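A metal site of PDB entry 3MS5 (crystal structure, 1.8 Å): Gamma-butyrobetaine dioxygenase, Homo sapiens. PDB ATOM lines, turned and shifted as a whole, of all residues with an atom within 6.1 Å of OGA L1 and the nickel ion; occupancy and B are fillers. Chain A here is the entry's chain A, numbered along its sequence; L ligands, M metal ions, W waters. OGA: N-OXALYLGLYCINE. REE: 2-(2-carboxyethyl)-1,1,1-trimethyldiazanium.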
ATOM      1  N   TRP A 182      20.508 -25.313  18.083  1.00  0.00           N
ATOM      2  CA  TRP A 182      19.831 -24.046  17.776  1.00  0.00           C
ATOM      3  C   TRP A 182      20.789 -22.968  17.338  1.00  0.00           C
ATOM      4  O   TRP A 182      21.986 -22.984  17.683  1.00  0.00           O
ATOM      5  CB  TRP A 182      18.978 -23.551  18.924  1.00  0.00           C
ATOM      6  CG  TRP A 182      19.482 -23.920  20.266  1.00  0.00           C
ATOM      7  CD1 TRP A 182      19.080 -25.022  20.969  1.00  0.00           C
ATOM      8  CD2 TRP A 182      20.428 -23.236  21.111  1.00  0.00           C
ATOM      9  NE1 TRP A 182      19.737 -25.079  22.165  1.00  0.00           N
ATOM     10  CE2 TRP A 182      20.572 -24.010  22.303  1.00  0.00           C
ATOM     11  CE3 TRP A 182      21.179 -22.068  20.999  1.00  0.00           C
ATOM     12  CZ2 TRP A 182      21.397 -23.648  23.363  1.00  0.00           C
ATOM     13  CZ3 TRP A 182      22.034 -21.707  22.054  1.00  0.00           C
ATOM     14  CH2 TRP A 182      22.119 -22.506  23.230  1.00  0.00           C
ATOM     15  N   VAL A 184      21.974 -19.171  17.245  1.00  0.00           N
ATOM     16  CA  VAL A 184      21.888 -17.831  17.854  1.00  0.00           C
ATOM     17  C   VAL A 184      22.309 -16.824  16.810  1.00  0.00           C
ATOM     18  O   VAL A 184      23.497 -16.659  16.512  1.00  0.00           O
ATOM     19  CB  VAL A 184      22.775 -17.711  19.075  1.00  0.00           C
ATOM     20  CG1 VAL A 184      22.562 -16.302  19.757  1.00  0.00           C
ATOM     21  CG2 VAL A 184      22.506 -18.898  20.084  1.00  0.00           C
ATOM     22  N   ASN A 192      12.613 -15.341  20.614  1.00  0.00           N
ATOM     23  CA  ASN A 192      13.378 -15.313  21.846  1.00  0.00           C
ATOM     24  C   ASN A 192      14.327 -14.109  21.808  1.00  0.00           C
ATOM     25  O   ASN A 192      14.877 -13.795  20.765  1.00  0.00           O
ATOM     26  CB  ASN A 192      14.153 -16.637  22.025  1.00  0.00           C
ATOM     27  CG  ASN A 192      14.698 -16.831  23.441  1.00  0.00           C
ATOM     28  OD1 ASN A 192      15.690 -16.213  23.826  1.00  0.00           O
ATOM     29  ND2 ASN A 192      14.063 -17.733  24.216  1.00  0.00           N
ATOM     30  N   ALA A 194      17.131 -13.878  22.692  1.00  0.00           N
ATOM     31  CA  ALA A 194      18.432 -14.360  22.223  1.00  0.00           C
ATOM     32  C   ALA A 194      18.675 -14.110  20.728  1.00  0.00           C
ATOM     33  O   ALA A 194      19.795 -13.847  20.300  1.00  0.00           O
ATOM     34  CB  ALA A 194      18.598 -15.890  22.545  1.00  0.00           C
ATOM     35  N   TYR A 195      17.615 -14.204  19.948  1.00  0.00           N
ATOM     36  CA  TYR A 195      17.708 -14.204  18.487  1.00  0.00           C
ATOM     37  C   TYR A 195      17.507 -12.759  17.967  1.00  0.00           C
ATOM     38  O   TYR A 195      16.774 -12.541  17.008  1.00  0.00           O
ATOM     39  CB  TYR A 195      16.707 -15.172  17.900  1.00  0.00           C
ATOM     40  CG  TYR A 195      16.848 -16.619  18.349  1.00  0.00           C
ATOM     41  CD1 TYR A 195      18.073 -17.129  18.800  1.00  0.00           C
ATOM     42  CD2 TYR A 195      15.773 -17.506  18.288  1.00  0.00           C
ATOM     43  CE1 TYR A 195      18.226 -18.485  19.183  1.00  0.00           C
ATOM     44  CE2 TYR A 195      15.913 -18.845  18.720  1.00  0.00           C
ATOM     45  CZ  TYR A 195      17.167 -19.314  19.116  1.00  0.00           C
ATOM     46  OH  TYR A 195      17.362 -20.623  19.492  1.00  0.00           O
ATOM     47  N   LEU A 200      22.238  -9.473  26.228  1.00  0.00           N
ATOM     48  CA  LEU A 200      21.591 -10.427  27.144  1.00  0.00           C
ATOM     49  C   LEU A 200      22.301 -10.235  28.465  1.00  0.00           C
ATOM     50  O   LEU A 200      23.536 -10.345  28.509  1.00  0.00           O
ATOM     51  CB  LEU A 200      21.758 -11.867  26.633  1.00  0.00           C
ATOM     52  CG  LEU A 200      21.215 -12.212  25.233  1.00  0.00           C
ATOM     53  CD1 LEU A 200      21.394 -13.686  24.886  1.00  0.00           C
ATOM     54  CD2 LEU A 200      19.710 -11.840  25.229  1.00  0.00           C
ATOM     55  N   HIS A 203      21.935 -14.584  32.722  1.00  0.00           N
ATOM     56  CA  HIS A 203      20.835 -15.518  32.802  1.00  0.00           C
ATOM     57  C   HIS A 203      21.400 -16.931  32.845  1.00  0.00           C
ATOM     58  O   HIS A 203      22.572 -17.172  32.478  1.00  0.00           O
ATOM     59  CB  HIS A 203      19.879 -15.389  31.630  1.00  0.00           C
ATOM     60  CG  HIS A 203      20.482 -15.719  30.317  1.00  0.00           C
ATOM     61  ND1 HIS A 203      21.281 -14.844  29.624  1.00  0.00           N
ATOM     62  CD2 HIS A 203      20.396 -16.838  29.543  1.00  0.00           C
ATOM     63  CE1 HIS A 203      21.666 -15.409  28.489  1.00  0.00           C
ATOM     64  NE2 HIS A 203      21.159 -16.627  28.429  1.00  0.00           N
ATOM     65  N   THR A 204      20.573 -17.838  33.345  1.00  0.00           N
ATOM     66  CA  THR A 204      20.652 -19.269  33.062  1.00  0.00           C
ATOM     67  C   THR A 204      19.674 -19.577  31.915  1.00  0.00           C
ATOM     68  O   THR A 204      18.687 -18.896  31.727  1.00  0.00           O
ATOM     69  CB  THR A 204      20.351 -20.123  34.318  1.00  0.00           C
ATOM     70  OG1 THR A 204      18.997 -19.938  34.742  1.00  0.00           O
ATOM     71  CG2 THR A 204      21.288 -19.804  35.484  1.00  0.00           C
ATOM     72  N   ASP A 205      19.981 -20.595  31.083  1.00  0.00           N
ATOM     73  CA  ASP A 205      19.078 -20.959  30.020  1.00  0.00           C
ATOM     74  C   ASP A 205      17.975 -21.830  30.524  1.00  0.00           C
ATOM     75  O   ASP A 205      18.177 -22.770  31.280  1.00  0.00           O
ATOM     76  CB  ASP A 205      19.768 -21.680  28.896  1.00  0.00           C
ATOM     77  CG  ASP A 205      20.358 -20.749  27.870  1.00  0.00           C
ATOM     78  OD1 ASP A 205      20.702 -19.596  28.180  1.00  0.00           O
ATOM     79  OD2 ASP A 205      20.490 -21.196  26.701  1.00  0.00           O
ATOM     80  N   GLN A 216      25.431 -26.669  28.883  1.00  0.00           N
ATOM     81  CA  GLN A 216      25.263 -25.962  27.640  1.00  0.00           C
ATOM     82  C   GLN A 216      26.511 -26.067  26.784  1.00  0.00           C
ATOM     83  O   GLN A 216      27.609 -25.943  27.279  1.00  0.00           O
ATOM     84  CB  GLN A 216      24.987 -24.475  27.963  1.00  0.00           C
ATOM     85  CG  GLN A 216      24.439 -23.755  26.823  1.00  0.00           C
ATOM     86  CD  GLN A 216      24.132 -22.299  27.098  1.00  0.00           C
ATOM     87  OE1 GLN A 216      24.460 -21.513  26.278  1.00  0.00           O
ATOM     88  NE2 GLN A 216      23.455 -21.968  28.234  1.00  0.00           N
ATOM     89  N   LEU A 218      28.194 -24.174  23.328  1.00  0.00           N
ATOM     90  CA  LEU A 218      28.004 -23.018  22.427  1.00  0.00           C
ATOM     91  C   LEU A 218      29.214 -22.861  21.540  1.00  0.00           C
ATOM     92  O   LEU A 218      30.320 -22.664  22.029  1.00  0.00           O
ATOM     93  CB  LEU A 218      27.786 -21.688  23.187  1.00  0.00           C
ATOM     94  CG  LEU A 218      26.462 -21.246  23.782  1.00  0.00           C
ATOM     95  CD1 LEU A 218      26.663 -19.846  24.493  1.00  0.00           C
ATOM     96  CD2 LEU A 218      25.366 -21.181  22.756  1.00  0.00           C
ATOM     97  N   GLY A 228      29.067  -8.031  20.885  1.00  0.00           N
ATOM     98  CA  GLY A 228      28.859  -9.448  21.127  1.00  0.00           C
ATOM     99  C   GLY A 228      29.885 -10.202  21.950  1.00  0.00           C
ATOM    100  O   GLY A 228      29.990 -11.419  21.832  1.00  0.00           O
ATOM    101  N   ASP A 229      30.653  -9.482  22.778  1.00  0.00           N
ATOM    102  CA  ASP A 229      31.515 -10.188  23.712  1.00  0.00           C
ATOM    103  C   ASP A 229      30.700 -10.975  24.726  1.00  0.00           C
ATOM    104  O   ASP A 229      29.492 -10.705  24.956  1.00  0.00           O
ATOM    105  CB  ASP A 229      32.511  -9.225  24.366  1.00  0.00           C
ATOM    106  CG  ASP A 229      33.484  -8.612  23.358  1.00  0.00           C
ATOM    107  OD1 ASP A 229      33.558  -9.108  22.213  1.00  0.00           O
ATOM    108  OD2 ASP A 229      34.179  -7.637  23.713  1.00  0.00           O
ATOM    109  N   SER A 230      31.348 -11.994  25.300  1.00  0.00           N
ATOM    110  CA  SER A 230      30.769 -12.939  26.233  1.00  0.00           C
ATOM    111  C   SER A 230      31.094 -12.546  27.649  1.00  0.00           C
ATOM    112  O   SER A 230      32.170 -11.999  27.919  1.00  0.00           O
ATOM    113  CB  SER A 230      31.314 -14.345  25.974  1.00  0.00           C
ATOM    114  OG  SER A 230      31.112 -14.715  24.638  1.00  0.00           O
ATOM    115  N   MET A 333      34.552 -14.698  21.978  1.00  0.00           N
ATOM    116  CA  MET A 333      34.575 -15.959  21.212  1.00  0.00           C
ATOM    117  C   MET A 333      34.951 -15.661  19.777  1.00  0.00           C
ATOM    118  O   MET A 333      34.410 -14.712  19.185  1.00  0.00           O
ATOM    119  CB  MET A 333      33.219 -16.694  21.267  1.00  0.00           C
ATOM    120  CG  MET A 333      32.862 -17.181  22.680  1.00  0.00           C
ATOM    121  SD  MET A 333      31.485 -18.288  22.712  1.00  0.00           S
ATOM    122  CE  MET A 333      32.293 -19.789  21.967  1.00  0.00           C
ATOM    123  N   PHE A 341      29.669 -25.529  29.448  1.00  0.00           N
ATOM    124  CA  PHE A 341      29.537 -25.026  30.817  1.00  0.00           C
ATOM    125  C   PHE A 341      28.340 -25.511  31.590  1.00  0.00           C
ATOM    126  O   PHE A 341      27.365 -26.021  31.025  1.00  0.00           O
ATOM    127  CB  PHE A 341      29.653 -23.495  30.867  1.00  0.00           C
ATOM    128  CG  PHE A 341      28.576 -22.737  30.166  1.00  0.00           C
ATOM    129  CD1 PHE A 341      27.432 -22.289  30.864  1.00  0.00           C
ATOM    130  CD2 PHE A 341      28.743 -22.351  28.841  1.00  0.00           C
ATOM    131  CE1 PHE A 341      26.481 -21.495  30.211  1.00  0.00           C
ATOM    132  CE2 PHE A 341      27.778 -21.608  28.177  1.00  0.00           C
ATOM    133  CZ  PHE A 341      26.643 -21.175  28.876  1.00  0.00           C
ATOM    134  N   ASN A 343      25.195 -25.064  33.263  1.00  0.00           N
ATOM    135  CA  ASN A 343      24.040 -24.171  33.123  1.00  0.00           C
ATOM    136  C   ASN A 343      23.214 -24.053  34.409  1.00  0.00           C
ATOM    137  O   ASN A 343      22.403 -23.140  34.542  1.00  0.00           O
ATOM    138  CB  ASN A 343      23.161 -24.594  31.893  1.00  0.00           C
ATOM    139  CG  ASN A 343      21.970 -23.622  31.643  1.00  0.00           C
ATOM    140  OD1 ASN A 343      22.221 -22.420  31.359  1.00  0.00           O
ATOM    141  ND2 ASN A 343      20.699 -24.088  31.823  1.00  0.00           N
ATOM    142  N   HIS A 348      25.341 -16.464  32.420  1.00  0.00           N
ATOM    143  CA  HIS A 348      26.077 -16.029  31.222  1.00  0.00           C
ATOM    144  C   HIS A 348      25.279 -14.973  30.490  1.00  0.00           C
ATOM    145  O   HIS A 348      24.043 -14.784  30.701  1.00  0.00           O
ATOM    146  CB  HIS A 348      26.380 -17.206  30.309  1.00  0.00           C
ATOM    147  CG  HIS A 348      25.139 -17.852  29.739  1.00  0.00           C
ATOM    148  ND1 HIS A 348      24.285 -18.614  30.494  1.00  0.00           N
ATOM    149  CD2 HIS A 348      24.575 -17.753  28.508  1.00  0.00           C
ATOM    150  CE1 HIS A 348      23.242 -18.983  29.749  1.00  0.00           C
ATOM    151  NE2 HIS A 348      23.382 -18.461  28.535  1.00  0.00           N
ATOM    152  N   GLY A 349      25.991 -14.259  29.655  1.00  0.00           N
ATOM    153  CA  GLY A 349      25.391 -13.108  28.965  1.00  0.00           C
ATOM    154  C   GLY A 349      26.229 -12.689  27.784  1.00  0.00           C
ATOM    155  O   GLY A 349      27.305 -13.245  27.512  1.00  0.00           O
ATOM    156  N   ARG A 350      25.750 -11.661  27.062  1.00  0.00           N
ATOM    157  CA  ARG A 350      26.474 -11.210  25.913  1.00  0.00           C
ATOM    158  C   ARG A 350      26.158  -9.736  25.658  1.00  0.00           C
ATOM    159  O   ARG A 350      25.043  -9.289  25.918  1.00  0.00           O
ATOM    160  CB  ARG A 350      26.145 -12.040  24.657  1.00  0.00           C
ATOM    161  CG  ARG A 350      24.760 -11.929  24.150  1.00  0.00           C
ATOM    162  CD  ARG A 350      24.702 -11.525  22.688  1.00  0.00           C
ATOM    163  NE  ARG A 350      23.345 -11.089  22.355  1.00  0.00           N
ATOM    164  CZ  ARG A 350      22.392 -11.839  21.797  1.00  0.00           C
ATOM    165  NH1 ARG A 350      22.581 -13.089  21.433  1.00  0.00           N
ATOM    166  NH2 ARG A 350      21.210 -11.289  21.601  1.00  0.00           N
ATOM    167  N   ARG A 361      26.823 -12.477  12.827  1.00  0.00           N
ATOM    168  CA  ARG A 361      27.128 -13.236  14.037  1.00  0.00           C
ATOM    169  C   ARG A 361      26.249 -14.482  14.108  1.00  0.00           C
ATOM    170  O   ARG A 361      25.040 -14.399  13.949  1.00  0.00           O
ATOM    171  CB  ARG A 361      26.891 -12.357  15.266  1.00  0.00           C
ATOM    172  CG  ARG A 361      27.459 -12.945  16.540  1.00  0.00           C
ATOM    173  CD  ARG A 361      27.201 -11.975  17.691  1.00  0.00           C
ATOM    174  NE  ARG A 361      27.802 -12.372  18.944  1.00  0.00           N
ATOM    175  CZ  ARG A 361      27.286 -13.186  19.883  1.00  0.00           C
ATOM    176  NH1 ARG A 361      26.090 -13.770  19.775  1.00  0.00           N
ATOM    177  NH2 ARG A 361      27.999 -13.385  20.994  1.00  0.00           N
ATOM    178  N   LEU A 363      26.172 -18.303  16.420  1.00  0.00           N
ATOM    179  CA  LEU A 363      26.616 -19.367  17.313  1.00  0.00           C
ATOM    180  C   LEU A 363      25.646 -20.551  17.148  1.00  0.00           C
ATOM    181  O   LEU A 363      24.437 -20.334  16.945  1.00  0.00           O
ATOM    182  CB  LEU A 363      26.591 -18.919  18.777  1.00  0.00           C
ATOM    183  CG  LEU A 363      27.092 -17.517  19.155  1.00  0.00           C
ATOM    184  CD1 LEU A 363      27.010 -17.370  20.749  1.00  0.00           C
ATOM    185  CD2 LEU A 363      28.499 -17.325  18.639  1.00  0.00           C
ATOM    186  N   TYR A 367      22.231 -28.481  24.343  1.00  0.00           N
ATOM    187  CA  TYR A 367      22.204 -28.841  25.745  1.00  0.00           C
ATOM    188  C   TYR A 367      22.493 -30.321  25.969  1.00  0.00           C
ATOM    189  O   TYR A 367      22.194 -31.163  25.108  1.00  0.00           O
ATOM    190  CB  TYR A 367      20.827 -28.523  26.325  1.00  0.00           C
ATOM    191  CG  TYR A 367      20.350 -27.068  26.190  1.00  0.00           C
ATOM    192  CD1 TYR A 367      21.042 -26.015  26.785  1.00  0.00           C
ATOM    193  CD2 TYR A 367      19.169 -26.758  25.512  1.00  0.00           C
ATOM    194  CE1 TYR A 367      20.617 -24.711  26.661  1.00  0.00           C
ATOM    195  CE2 TYR A 367      18.681 -25.444  25.416  1.00  0.00           C
ATOM    196  CZ  TYR A 367      19.408 -24.416  26.011  1.00  0.00           C
ATOM    197  OH  TYR A 367      18.968 -23.109  25.874  1.00  0.00           O
HETATM  198  C1  OGA L   1      21.404 -17.432  24.582  1.00  0.00           C
HETATM  199  C2  OGA L   1      22.807 -16.921  24.897  1.00  0.00           C
HETATM  200  C4  OGA L   1      24.929 -15.924  24.204  1.00  0.00           C
HETATM  201  C5  OGA L   1      25.515 -15.203  22.974  1.00  0.00           C
HETATM  202  O1  OGA L   1      21.139 -17.539  23.371  1.00  0.00           O
HETATM  203  O2  OGA L   1      20.682 -17.808  25.529  1.00  0.00           O
HETATM  204  O2' OGA L   1      23.143 -16.876  26.058  1.00  0.00           O
HETATM  205  O3  OGA L   1      24.756 -14.919  22.015  1.00  0.00           O
HETATM  206  N1  OGA L   1      23.599 -16.497  23.896  1.00  0.00           N
HETATM  207  O4  OGA L   1      26.734 -14.957  23.048  1.00  0.00           O
HETATM  208  C1  REE L   2      15.799 -19.258  27.533  1.00  0.00           C
HETATM  209  N1  REE L   2      17.354 -20.391  24.861  1.00  0.00           N
HETATM  210  O1  REE L   2      14.894 -19.002  26.723  1.00  0.00           O
HETATM  211  C2  REE L   2      17.249 -19.262  27.057  1.00  0.00           C
HETATM  212  N2  REE L   2      17.719 -20.433  23.463  1.00  0.00           N
HETATM  213  O2  REE L   2      15.664 -19.341  28.789  1.00  0.00           O
HETATM  214  C3  REE L   2      17.548 -19.134  25.560  1.00  0.00           C
HETATM  215  C4  REE L   2      17.543 -21.844  23.047  1.00  0.00           C
HETATM  216  C5  REE L   2      16.768 -19.617  22.661  1.00  0.00           C
HETATM  217  C6  REE L   2      19.082 -19.955  23.210  1.00  0.00           C
HETATM  218 NI    NI M   1      21.890 -18.127  27.153  1.00  0.00          NI
HETATM  219  O   HOH W   1      22.608 -19.617  25.847  1.00  0.00           O
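The nickel ion is bound by an oxygen (O2) of OGA L1 (2.0 Å), a ring nitrogen (NE2) of His 348 (2.1 Å), an oxygen (O2') of OGA L1 (2.1 Å), a ring nitrogen (NE2) of His 203 (2.1 Å), water W1 (2.1 Å) and the side-chain carboxylate of Asp 205 (2.2 Å).
OD1 of Asn 192 lies close to N of Ala 194 (3.0 Å). NH2 of Arg 361 sits at hydrogen-bond distance from O of Gly 228 (2.9 Å). The side-chain carboxylate (OD2) of Asp 205 lies close to the side-chain amide nitrogen (NE2) of Gln 216 (3.4 Å). ND2 of Asn 343 sits at hydrogen-bond distance from O of Asp 205, at 2.9 Å. The side-chain carboxylate (OD2) of Asp 205 sits at hydrogen-bond distance from the side-chain hydroxyl (OH) of Tyr 367 (2.6 Å). The backbone carbonyl oxygen (O) of Leu 363 lies within hydrogen-bond range of the backbone NH (N) of Val 184. The guanidinium group (NH1) of Arg 350 sits at hydrogen-bond distance from the backbone carbonyl oxygen (O) of Ala 194 (3.1 Å). The backbone carbonyl oxygen (O) of Arg 350 sits at hydrogen-bond distance from the backbone NH (N) of Leu 200 (2.8 Å).
Of the 23 residues printed, 3 come within 4 Å of the nickel ion. The nearest printed residue that does not touch the nickel ion is Gln 216 (4.3 Å).
Water W1 lies within hydrogen-bond range of OE1 of Gln 216 (2.7 Å) and OD2 of Asp 205 (2.8 Å).
ND2 of Asn 192 lies within hydrogen-bond range of O1 of REE L2 (2.9 Å). An oxygen (O3) of OGA L1 lies within salt-bridge range of the guanidinium group (NH1) of Arg 350, at 2.9 Å. The guanidinium group (NH1) of Arg 361 lies within salt-bridge range of an oxygen (O3) of OGA L1, at 2.8 Å. N1 of REE L2 sits at hydrogen-bond distance from OH of Tyr 367 (3.3 Å).
Val 184 touches OGA L1. Ala 194 touches OGA L1 (CB to O1, 3.1 Å). Leu 200 touches OGA L1 (CD1 to C2, 3.5 Å). CD1 of Leu 363 touches O4 of OGA L1, at 3.3 Å. Hydrophobic or aromatic side chains within 4 Å of OGA L1: Val 184, Ala 194, Leu 200, His 203, His 348 and Leu 363. Nine residues have an atom within 4 Å of OGA L1: Val 184, Ala 194, Leu 200, His 203, Asp 205, His 348, Arg 350, Arg 361 and Leu 363.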
